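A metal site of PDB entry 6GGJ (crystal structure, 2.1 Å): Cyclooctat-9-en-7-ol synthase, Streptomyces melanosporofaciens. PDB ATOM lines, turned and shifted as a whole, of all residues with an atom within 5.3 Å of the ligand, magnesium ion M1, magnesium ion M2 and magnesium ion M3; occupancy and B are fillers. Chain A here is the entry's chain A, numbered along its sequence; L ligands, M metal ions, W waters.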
ATOM      1  N   ASN A 103     -28.892  18.497  18.514  1.00  0.00           N
ATOM      2  CA  ASN A 103     -28.783  17.287  19.326  1.00  0.00           C
ATOM      3  C   ASN A 103     -29.898  16.302  19.017  1.00  0.00           C
ATOM      4  O   ASN A 103     -29.656  15.094  18.885  1.00  0.00           O
ATOM      5  CB  ASN A 103     -28.768  17.627  20.808  1.00  0.00           C
ATOM      6  CG  ASN A 103     -28.045  16.567  21.616  1.00  0.00           C
ATOM      7  OD1 ASN A 103     -28.672  15.789  22.342  1.00  0.00           O
ATOM      8  ND2 ASN A 103     -26.725  16.508  21.480  1.00  0.00           N
ATOM      9  N   THR A 106     -29.415  14.591  15.484  1.00  0.00           N
ATOM     10  CA  THR A 106     -28.305  13.630  15.442  1.00  0.00           C
ATOM     11  C   THR A 106     -28.602  12.407  16.306  1.00  0.00           C
ATOM     12  O   THR A 106     -28.110  11.316  16.006  1.00  0.00           O
ATOM     13  CB  THR A 106     -26.988  14.309  15.829  1.00  0.00           C
ATOM     14  OG1 THR A 106     -27.074  14.946  17.105  1.00  0.00           O
ATOM     15  CG2 THR A 106     -26.627  15.358  14.777  1.00  0.00           C
ATOM     16  N   PHE A 107     -29.451  12.554  17.325  1.00  0.00           N
ATOM     17  CA  PHE A 107     -30.022  11.385  18.005  1.00  0.00           C
ATOM     18  C   PHE A 107     -30.742  10.479  17.015  1.00  0.00           C
ATOM     19  O   PHE A 107     -30.525   9.259  16.990  1.00  0.00           O
ATOM     20  CB  PHE A 107     -30.968  11.848  19.109  1.00  0.00           C
ATOM     21  CG  PHE A 107     -30.470  11.630  20.503  1.00  0.00           C
ATOM     22  CD1 PHE A 107     -30.343  10.342  21.012  1.00  0.00           C
ATOM     23  CD2 PHE A 107     -30.166  12.710  21.316  1.00  0.00           C
ATOM     24  CE1 PHE A 107     -29.882  10.141  22.312  1.00  0.00           C
ATOM     25  CE2 PHE A 107     -29.711  12.517  22.616  1.00  0.00           C
ATOM     26  CZ  PHE A 107     -29.581  11.230  23.115  1.00  0.00           C
ATOM     27  N   ASP A 110     -28.413   8.602  15.064  1.00  0.00           N
ATOM     28  CA  ASP A 110     -27.758   7.567  15.865  1.00  0.00           C
ATOM     29  C   ASP A 110     -28.578   6.281  15.864  1.00  0.00           C
ATOM     30  O   ASP A 110     -28.025   5.180  15.710  1.00  0.00           O
ATOM     31  CB  ASP A 110     -27.544   8.081  17.290  1.00  0.00           C
ATOM     32  CG  ASP A 110     -26.678   7.147  18.131  1.00  0.00           C
ATOM     33  OD1 ASP A 110     -25.470   7.049  17.836  1.00  0.00           O
ATOM     34  OD2 ASP A 110     -27.200   6.528  19.075  1.00  0.00           O
ATOM     35  N   ASP A 111     -29.889   6.397  16.033  1.00  0.00           N
ATOM     36  CA  ASP A 111     -30.813   5.263  16.109  1.00  0.00           C
ATOM     37  C   ASP A 111     -31.212   4.696  14.746  1.00  0.00           C
ATOM     38  O   ASP A 111     -31.915   3.685  14.709  1.00  0.00           O
ATOM     39  CB  ASP A 111     -32.078   5.665  16.870  1.00  0.00           C
ATOM     40  CG  ASP A 111     -31.858   5.747  18.374  1.00  0.00           C
ATOM     41  OD1 ASP A 111     -31.116   4.893  18.913  1.00  0.00           O
ATOM     42  OD2 ASP A 111     -32.413   6.667  19.018  1.00  0.00           O
ATOM     43  N   PHE A 149     -19.594  14.371  13.146  1.00  0.00           N
ATOM     44  CA  PHE A 149     -20.272  13.405  14.005  1.00  0.00           C
ATOM     45  C   PHE A 149     -21.096  12.388  13.198  1.00  0.00           C
ATOM     46  O   PHE A 149     -21.013  11.176  13.440  1.00  0.00           O
ATOM     47  CB  PHE A 149     -21.192  14.102  15.018  1.00  0.00           C
ATOM     48  CG  PHE A 149     -22.028  13.131  15.796  1.00  0.00           C
ATOM     49  CD1 PHE A 149     -21.474  12.420  16.862  1.00  0.00           C
ATOM     50  CD2 PHE A 149     -23.343  12.883  15.437  1.00  0.00           C
ATOM     51  CE1 PHE A 149     -22.205  11.506  17.575  1.00  0.00           C
ATOM     52  CE2 PHE A 149     -24.107  11.960  16.150  1.00  0.00           C
ATOM     53  CZ  PHE A 149     -23.530  11.265  17.225  1.00  0.00           C
ATOM     54  N   ASP A 153     -20.369   8.368  12.919  1.00  0.00           N
ATOM     55  CA  ASP A 153     -21.324   7.340  13.310  1.00  0.00           C
ATOM     56  C   ASP A 153     -21.587   6.378  12.147  1.00  0.00           C
ATOM     57  O   ASP A 153     -21.644   5.162  12.323  1.00  0.00           O
ATOM     58  CB  ASP A 153     -22.613   8.005  13.809  1.00  0.00           C
ATOM     59  CG  ASP A 153     -23.749   7.009  13.990  1.00  0.00           C
ATOM     60  OD1 ASP A 153     -23.612   6.089  14.827  1.00  0.00           O
ATOM     61  OD2 ASP A 153     -24.812   7.165  13.309  1.00  0.00           O
ATOM     62  N   ARG A 177     -14.671   7.477  22.044  1.00  0.00           N
ATOM     63  CA  ARG A 177     -15.926   8.112  22.453  1.00  0.00           C
ATOM     64  C   ARG A 177     -15.857   9.629  22.468  1.00  0.00           C
ATOM     65  O   ARG A 177     -16.917  10.274  22.378  1.00  0.00           O
ATOM     66  CB  ARG A 177     -16.327   7.579  23.821  1.00  0.00           C
ATOM     67  CG  ARG A 177     -16.697   6.113  23.720  1.00  0.00           C
ATOM     68  CD  ARG A 177     -17.998   6.021  22.914  1.00  0.00           C
ATOM     69  NE  ARG A 177     -19.129   5.693  23.778  1.00  0.00           N
ATOM     70  CZ  ARG A 177     -20.401   6.007  23.525  1.00  0.00           C
ATOM     71  NH1 ARG A 177     -20.739   6.648  22.409  1.00  0.00           N
ATOM     72  NH2 ARG A 177     -21.347   5.674  24.393  1.00  0.00           N
ATOM     73  N   ASP A 180     -17.302   9.862  19.272  1.00  0.00           N
ATOM     74  CA  ASP A 180     -18.447   9.036  18.915  1.00  0.00           C
ATOM     75  C   ASP A 180     -19.654   9.327  19.793  1.00  0.00           C
ATOM     76  O   ASP A 180     -20.802   9.301  19.311  1.00  0.00           O
ATOM     77  CB  ASP A 180     -18.108   7.565  18.973  1.00  0.00           C
ATOM     78  CG  ASP A 180     -19.335   6.695  18.848  1.00  0.00           C
ATOM     79  OD1 ASP A 180     -19.830   6.539  17.712  1.00  0.00           O
ATOM     80  OD2 ASP A 180     -19.822   6.205  19.888  1.00  0.00           O
ATOM     81  N   ILE A 181     -19.445   9.622  21.084  1.00  0.00           N
ATOM     82  CA  ILE A 181     -20.578   9.939  21.926  1.00  0.00           C
ATOM     83  C   ILE A 181     -21.175  11.297  21.567  1.00  0.00           C
ATOM     84  O   ILE A 181     -22.315  11.582  21.935  1.00  0.00           O
ATOM     85  CB  ILE A 181     -20.230   9.866  23.423  1.00  0.00           C
ATOM     86  CG1 ILE A 181     -21.524   9.688  24.229  1.00  0.00           C
ATOM     87  CG2 ILE A 181     -19.508  11.146  23.870  1.00  0.00           C
ATOM     88  CD1 ILE A 181     -21.321   9.252  25.643  1.00  0.00           C
ATOM     89  N   GLY A 182     -20.429  12.136  20.857  1.00  0.00           N
ATOM     90  CA  GLY A 182     -20.928  13.438  20.456  1.00  0.00           C
ATOM     91  C   GLY A 182     -20.500  14.608  21.312  1.00  0.00           C
ATOM     92  O   GLY A 182     -20.961  15.738  21.055  1.00  0.00           O
ATOM     93  N   ASN A 220     -23.726   7.184  30.554  1.00  0.00           N
ATOM     94  CA  ASN A 220     -24.514   6.663  29.436  1.00  0.00           C
ATOM     95  C   ASN A 220     -24.288   5.183  29.223  1.00  0.00           C
ATOM     96  O   ASN A 220     -25.236   4.439  28.941  1.00  0.00           O
ATOM     97  CB  ASN A 220     -24.175   7.415  28.148  1.00  0.00           C
ATOM     98  CG  ASN A 220     -24.852   6.783  26.931  1.00  0.00           C
ATOM     99  OD1 ASN A 220     -24.247   5.969  26.235  1.00  0.00           O
ATOM    100  ND2 ASN A 220     -26.109   7.135  26.699  1.00  0.00           N
ATOM    101  N   ASP A 221     -23.037   4.721  29.318  1.00  0.00           N
ATOM    102  CA  ASP A 221     -22.776   3.313  29.085  1.00  0.00           C
ATOM    103  C   ASP A 221     -23.531   2.447  30.075  1.00  0.00           C
ATOM    104  O   ASP A 221     -24.082   1.404  29.710  1.00  0.00           O
ATOM    105  CB  ASP A 221     -21.280   3.022  29.147  1.00  0.00           C
ATOM    106  CG  ASP A 221     -20.551   3.437  27.885  1.00  0.00           C
ATOM    107  OD1 ASP A 221     -21.204   3.978  26.972  1.00  0.00           O
ATOM    108  OD2 ASP A 221     -19.311   3.254  27.842  1.00  0.00           O
ATOM    109  N   SER A 224     -27.447   2.602  29.326  1.00  0.00           N
ATOM    110  CA  SER A 224     -27.815   2.156  27.991  1.00  0.00           C
ATOM    111  C   SER A 224     -27.205   0.803  27.644  1.00  0.00           C
ATOM    112  O   SER A 224     -27.350   0.342  26.515  1.00  0.00           O
ATOM    113  CB  SER A 224     -27.418   3.207  26.941  1.00  0.00           C
ATOM    114  OG  SER A 224     -26.043   3.125  26.596  1.00  0.00           O
ATOM    115  N   ARG A 227     -30.074  -1.884  26.409  1.00  0.00           N
ATOM    116  CA  ARG A 227     -30.517  -1.663  25.033  1.00  0.00           C
ATOM    117  C   ARG A 227     -29.453  -2.098  24.034  1.00  0.00           C
ATOM    118  O   ARG A 227     -29.729  -2.884  23.119  1.00  0.00           O
ATOM    119  CB  ARG A 227     -30.870  -0.199  24.811  1.00  0.00           C
ATOM    120  CG  ARG A 227     -30.804   0.191  23.336  1.00  0.00           C
ATOM    121  CD  ARG A 227     -31.589   1.458  23.052  1.00  0.00           C
ATOM    122  NE  ARG A 227     -31.201   2.565  23.928  1.00  0.00           N
ATOM    123  CZ  ARG A 227     -30.118   3.327  23.746  1.00  0.00           C
ATOM    124  NH1 ARG A 227     -29.299   3.098  22.724  1.00  0.00           N
ATOM    125  NH2 ARG A 227     -29.867   4.323  24.581  1.00  0.00           N
ATOM    126  N   GLU A 228     -28.220  -1.602  24.195  1.00  0.00           N
ATOM    127  CA  GLU A 228     -27.203  -1.815  23.175  1.00  0.00           C
ATOM    128  C   GLU A 228     -26.761  -3.271  23.087  1.00  0.00           C
ATOM    129  O   GLU A 228     -26.435  -3.754  21.996  1.00  0.00           O
ATOM    130  CB  GLU A 228     -26.023  -0.873  23.435  1.00  0.00           C
ATOM    131  CG  GLU A 228     -26.461   0.607  23.443  1.00  0.00           C
ATOM    132  CD  GLU A 228     -25.421   1.588  23.962  1.00  0.00           C
ATOM    133  OE1 GLU A 228     -24.398   1.152  24.541  1.00  0.00           O
ATOM    134  OE2 GLU A 228     -25.630   2.813  23.778  1.00  0.00           O
ATOM    135  N   GLN A 233     -24.827  -3.871  19.873  1.00  0.00           N
ATOM    136  CA  GLN A 233     -23.927  -2.730  19.780  1.00  0.00           C
ATOM    137  C   GLN A 233     -22.783  -2.909  20.768  1.00  0.00           C
ATOM    138  O   GLN A 233     -23.003  -3.292  21.920  1.00  0.00           O
ATOM    139  CB  GLN A 233     -24.697  -1.433  20.047  1.00  0.00           C
ATOM    140  CG  GLN A 233     -25.417  -0.933  18.809  1.00  0.00           C
ATOM    141  CD  GLN A 233     -26.653  -0.108  19.128  1.00  0.00           C
ATOM    142  OE1 GLN A 233     -27.366  -0.395  20.077  1.00  0.00           O
ATOM    143  NE2 GLN A 233     -26.891   0.927  18.332  1.00  0.00           N
ATOM    144  N   THR A 235     -20.328  -0.509  21.444  1.00  0.00           N
ATOM    145  CA  THR A 235     -19.734   0.744  21.931  1.00  0.00           C
ATOM    146  C   THR A 235     -20.257   1.020  23.339  1.00  0.00           C
ATOM    147  O   THR A 235     -21.139   1.845  23.568  1.00  0.00           O
ATOM    148  CB  THR A 235     -20.031   1.874  20.961  1.00  0.00           C
ATOM    149  OG1 THR A 235     -19.522   1.509  19.672  1.00  0.00           O
ATOM    150  CG2 THR A 235     -19.366   3.175  21.414  1.00  0.00           C
ATOM    151  N   ASN A 236     -19.667   0.316  24.311  1.00  0.00           N
ATOM    152  CA  ASN A 236     -20.096   0.437  25.703  1.00  0.00           C
ATOM    153  C   ASN A 236     -19.027  -0.166  26.608  1.00  0.00           C
ATOM    154  O   ASN A 236     -18.744  -1.356  26.503  1.00  0.00           O
ATOM    155  CB  ASN A 236     -21.424  -0.276  25.911  1.00  0.00           C
ATOM    156  CG  ASN A 236     -22.035  -0.004  27.259  1.00  0.00           C
ATOM    157  OD1 ASN A 236     -21.470  -0.378  28.309  1.00  0.00           O
ATOM    158  ND2 ASN A 236     -23.195   0.650  27.267  1.00  0.00           N
ATOM    159  N   ARG A 294     -35.815   7.100  27.684  1.00  0.00           N
ATOM    160  CA  ARG A 294     -34.906   6.438  26.759  1.00  0.00           C
ATOM    161  C   ARG A 294     -34.220   5.243  27.394  1.00  0.00           C
ATOM    162  O   ARG A 294     -33.967   4.232  26.725  1.00  0.00           O
ATOM    163  CB  ARG A 294     -33.861   7.436  26.242  1.00  0.00           C
ATOM    164  CG  ARG A 294     -32.931   6.829  25.173  1.00  0.00           C
ATOM    165  CD  ARG A 294     -32.229   7.872  24.312  1.00  0.00           C
ATOM    166  NE  ARG A 294     -31.200   7.262  23.475  1.00  0.00           N
ATOM    167  CZ  ARG A 294     -31.395   6.809  22.236  1.00  0.00           C
ATOM    168  NH1 ARG A 294     -32.590   6.879  21.671  1.00  0.00           N
ATOM    169  NH2 ARG A 294     -30.381   6.271  21.555  1.00  0.00           N
ATOM    170  N   TYR A 295     -33.941   5.307  28.702  1.00  0.00           N
ATOM    171  CA  TYR A 295     -33.019   4.364  29.336  1.00  0.00           C
ATOM    172  C   TYR A 295     -33.685   3.518  30.421  1.00  0.00           C
ATOM    173  O   TYR A 295     -33.026   3.131  31.393  1.00  0.00           O
ATOM    174  CB  TYR A 295     -31.814   5.098  29.920  1.00  0.00           C
ATOM    175  CG  TYR A 295     -31.114   5.998  28.940  1.00  0.00           C
ATOM    176  CD1 TYR A 295     -30.323   5.467  27.914  1.00  0.00           C
ATOM    177  CD2 TYR A 295     -31.234   7.375  29.021  1.00  0.00           C
ATOM    178  CE1 TYR A 295     -29.683   6.281  27.006  1.00  0.00           C
ATOM    179  CE2 TYR A 295     -30.584   8.207  28.120  1.00  0.00           C
ATOM    180  CZ  TYR A 295     -29.803   7.646  27.107  1.00  0.00           C
ATOM    181  OH  TYR A 295     -29.155   8.465  26.203  1.00  0.00           O
HETATM  182  C1  LIG L   1     -25.728   9.806  22.120  1.00  0.00           C
HETATM  183  C2  LIG L   1     -25.966  10.618  20.852  1.00  0.00           C
HETATM  184  C3  LIG L   1     -26.569   8.536  22.020  1.00  0.00           C
HETATM  185  C4  LIG L   1     -26.020   7.562  23.052  1.00  0.00           C
HETATM  186  O1  LIG L   1     -28.555   7.190  23.934  1.00  0.00           O
HETATM  187  P1  LIG L   1     -27.347   6.364  23.532  1.00  0.00           P
HETATM  188  O2  LIG L   1     -26.907   5.504  24.686  1.00  0.00           O
HETATM  189  O3  LIG L   1     -27.645   5.451  22.366  1.00  0.00           O
HETATM  190  P2  LIG L   1     -24.594   6.639  22.341  1.00  0.00           P
HETATM  191  O4  LIG L   1     -23.432   7.607  22.419  1.00  0.00           O
HETATM  192  O5  LIG L   1     -24.348   5.404  23.183  1.00  0.00           O
HETATM  193  O6  LIG L   1     -24.802   6.214  20.902  1.00  0.00           O
HETATM  194  O7  LIG L   1     -25.551   8.274  24.164  1.00  0.00           O
HETATM  195  N1  LIG L   1     -25.576  11.985  21.134  1.00  0.00           N
HETATM  196 MG    MG M   1     -25.087   4.574  24.799  1.00  0.00          MG
HETATM  197 MG    MG M   2     -26.582   5.184  20.482  1.00  0.00          MG
HETATM  198 MG    MG M   3     -23.871   6.268  19.177  1.00  0.00          MG
HETATM  199  O   HOH W   1     -22.144   4.969  19.975  1.00  0.00           O
HETATM  200  O   HOH W   2     -24.967   4.290  18.616  1.00  0.00           O
HETATM  201  O   HOH W   3     -23.314   8.167  19.662  1.00  0.00           O
HETATM  202  O   HOH W   4     -27.058  10.237  25.433  1.00  0.00           O
HETATM  203  O   HOH W   5     -23.288   3.406  25.481  1.00  0.00           O
HETATM  204  O   HOH W   6     -22.713   3.661  22.033  1.00  0.00           O
HETATM  205  O   HOH W   7     -22.624   6.171  17.368  1.00  0.00           O
HETATM  206  O   HOH W   8     -28.440   3.871  19.503  1.00  0.00           O
HETATM  207  O   HOH W   9     -26.430   3.565  21.337  1.00  0.00           O
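The side-chain hydroxyl of Tyr 295 is in hydrogen-bond range of an oxygen (O1) of the ligand (2.7 Å). An oxygen (O1) of the ligand lies within salt-bridge range of the guanidinium group (NE) of Arg 294 (2.7 Å). The guanidinium group (NH1) of Arg 177 lies within salt-bridge range of an oxygen (O4) of the ligand. The guanidinium group (NH2) of Arg 227 is in salt-bridge range of an oxygen (O1) of the ligand, 3.2 Å away. O of Ile 181 lies within hydrogen-bond range of N1 of the ligand, at 3.4 Å.
The guanidinium group (NH1) of Arg 227 lies close to the side-chain carboxylate (OE2) of Glu 228. The backbone NH (N) of Gln 233 is in hydrogen-bond range of the backbone carbonyl oxygen (O) of Glu 228 (2.7 Å). OE1 of Glu 228 is in hydrogen-bond range of ND2 of Asn 236, 3.0 Å away. ND2 of Asn 220 is in hydrogen-bond range of OH of Tyr 295 (3.4 Å). OD1 of Asn 220 sits close to NH2 of Arg 177. The side-chain carboxylate of Asp 111 is in salt-bridge range of the guanidinium group of Arg 294 (2.7 Å). The guanidinium group of Arg 177 is in salt-bridge range of the side-chain carboxylate of Asp 180, at 2.7 Å. The guanidinium group (NH2) of Arg 177 lies within salt-bridge range of the side-chain carboxylate (OD1) of Asp 221 (3.1 Å).
CE1 of Phe 107 touches O1 of the ligand, at 3.6 Å. Ten residues have an atom within 4 Å of the ligand: Phe 107, Asp 110, Arg 177, Ile 181, Asn 220, Ser 224, Arg 227, Glu 228, Arg 294 and Tyr 295.
Merely in contact with magnesium ion M1: Arg 177. Four residues have an atom within 4 Å of magnesium ion M1: Arg 177, Asn 220, Ser 224 and Glu 228. The nearest printed residue that does not touch magnesium ion M1 is Asp 221 (4.5 Å).
One residue has an atom within 4 Å of magnesium ion M2: Asp 110.
Within 4 Å of magnesium ion M3: Asp 110.
O5 of the ligand is bound to magnesium ion M1, at 2.0 Å. Magnesium ion M1 is bound by O2 of the ligand (2.0 Å). OE2 of Glu 228 binds magnesium ion M1. OD1 of Asn 220 is bound to magnesium ion M1 (2.2 Å). Water W5 binds magnesium ion M1. OG of Ser 224 is bound to magnesium ion M1 (2.5 Å). Magnesium ion M1 has six donor atoms within binding distance.
Magnesium ion M2 is bound by water W9, at 1.8 Å. OD2 of Asp 110 is bound to magnesium ion M2, at 2.0 Å. Magnesium ion M2 is bound by O6 of the ligand. O3 of the ligand binds magnesium ion M2, 2.2 Å away. Water W8 is bound to magnesium ion M2 (2.5 Å). Magnesium ion M2 has five donor atoms within binding distance. Slightly farther from magnesium ion M2 lies water W2 (2.6 Å).
O6 of the ligand is bound to magnesium ion M3 (2.0 Å). Water W3 binds magnesium ion M3 (2.0 Å). Water W7 is bound to magnesium ion M3. OD1 of Asp 110 is bound to magnesium ion M3. Magnesium ion M3 is bound by water W1. Water W2 is bound to magnesium ion M3, at 2.3 Å. Magnesium ion M3 has six donor atoms within binding distance.
Water W8 lies within hydrogen-bond range of the side-chain carboxylate of Asp 111 and the guanidinium group of Arg 227. Water W7 lies within hydrogen-bond range of OD1 of Asp 153 (2.7 Å) and OD1 of Asp 180 (2.8 Å). Water W1 bridges OD2 of Asp 180 (2.6 Å) and NH1 of Arg 177 (3.3 Å). Water W3 lies within hydrogen-bond range of the backbone carbonyl oxygen of Asp 180 (2.8 Å) and an oxygen (O4) of the ligand (2.8 Å). Water W6 bridges O of Thr 235 and NH2 of Arg 177. Water W4 lies within hydrogen-bond range of an oxygen (O7) of the ligand (2.8 Å), the side-chain hydroxyl (OH) of Tyr 295 (2.9 Å) and the side-chain amide nitrogen (ND2) of Asn 220 (3.5 Å).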
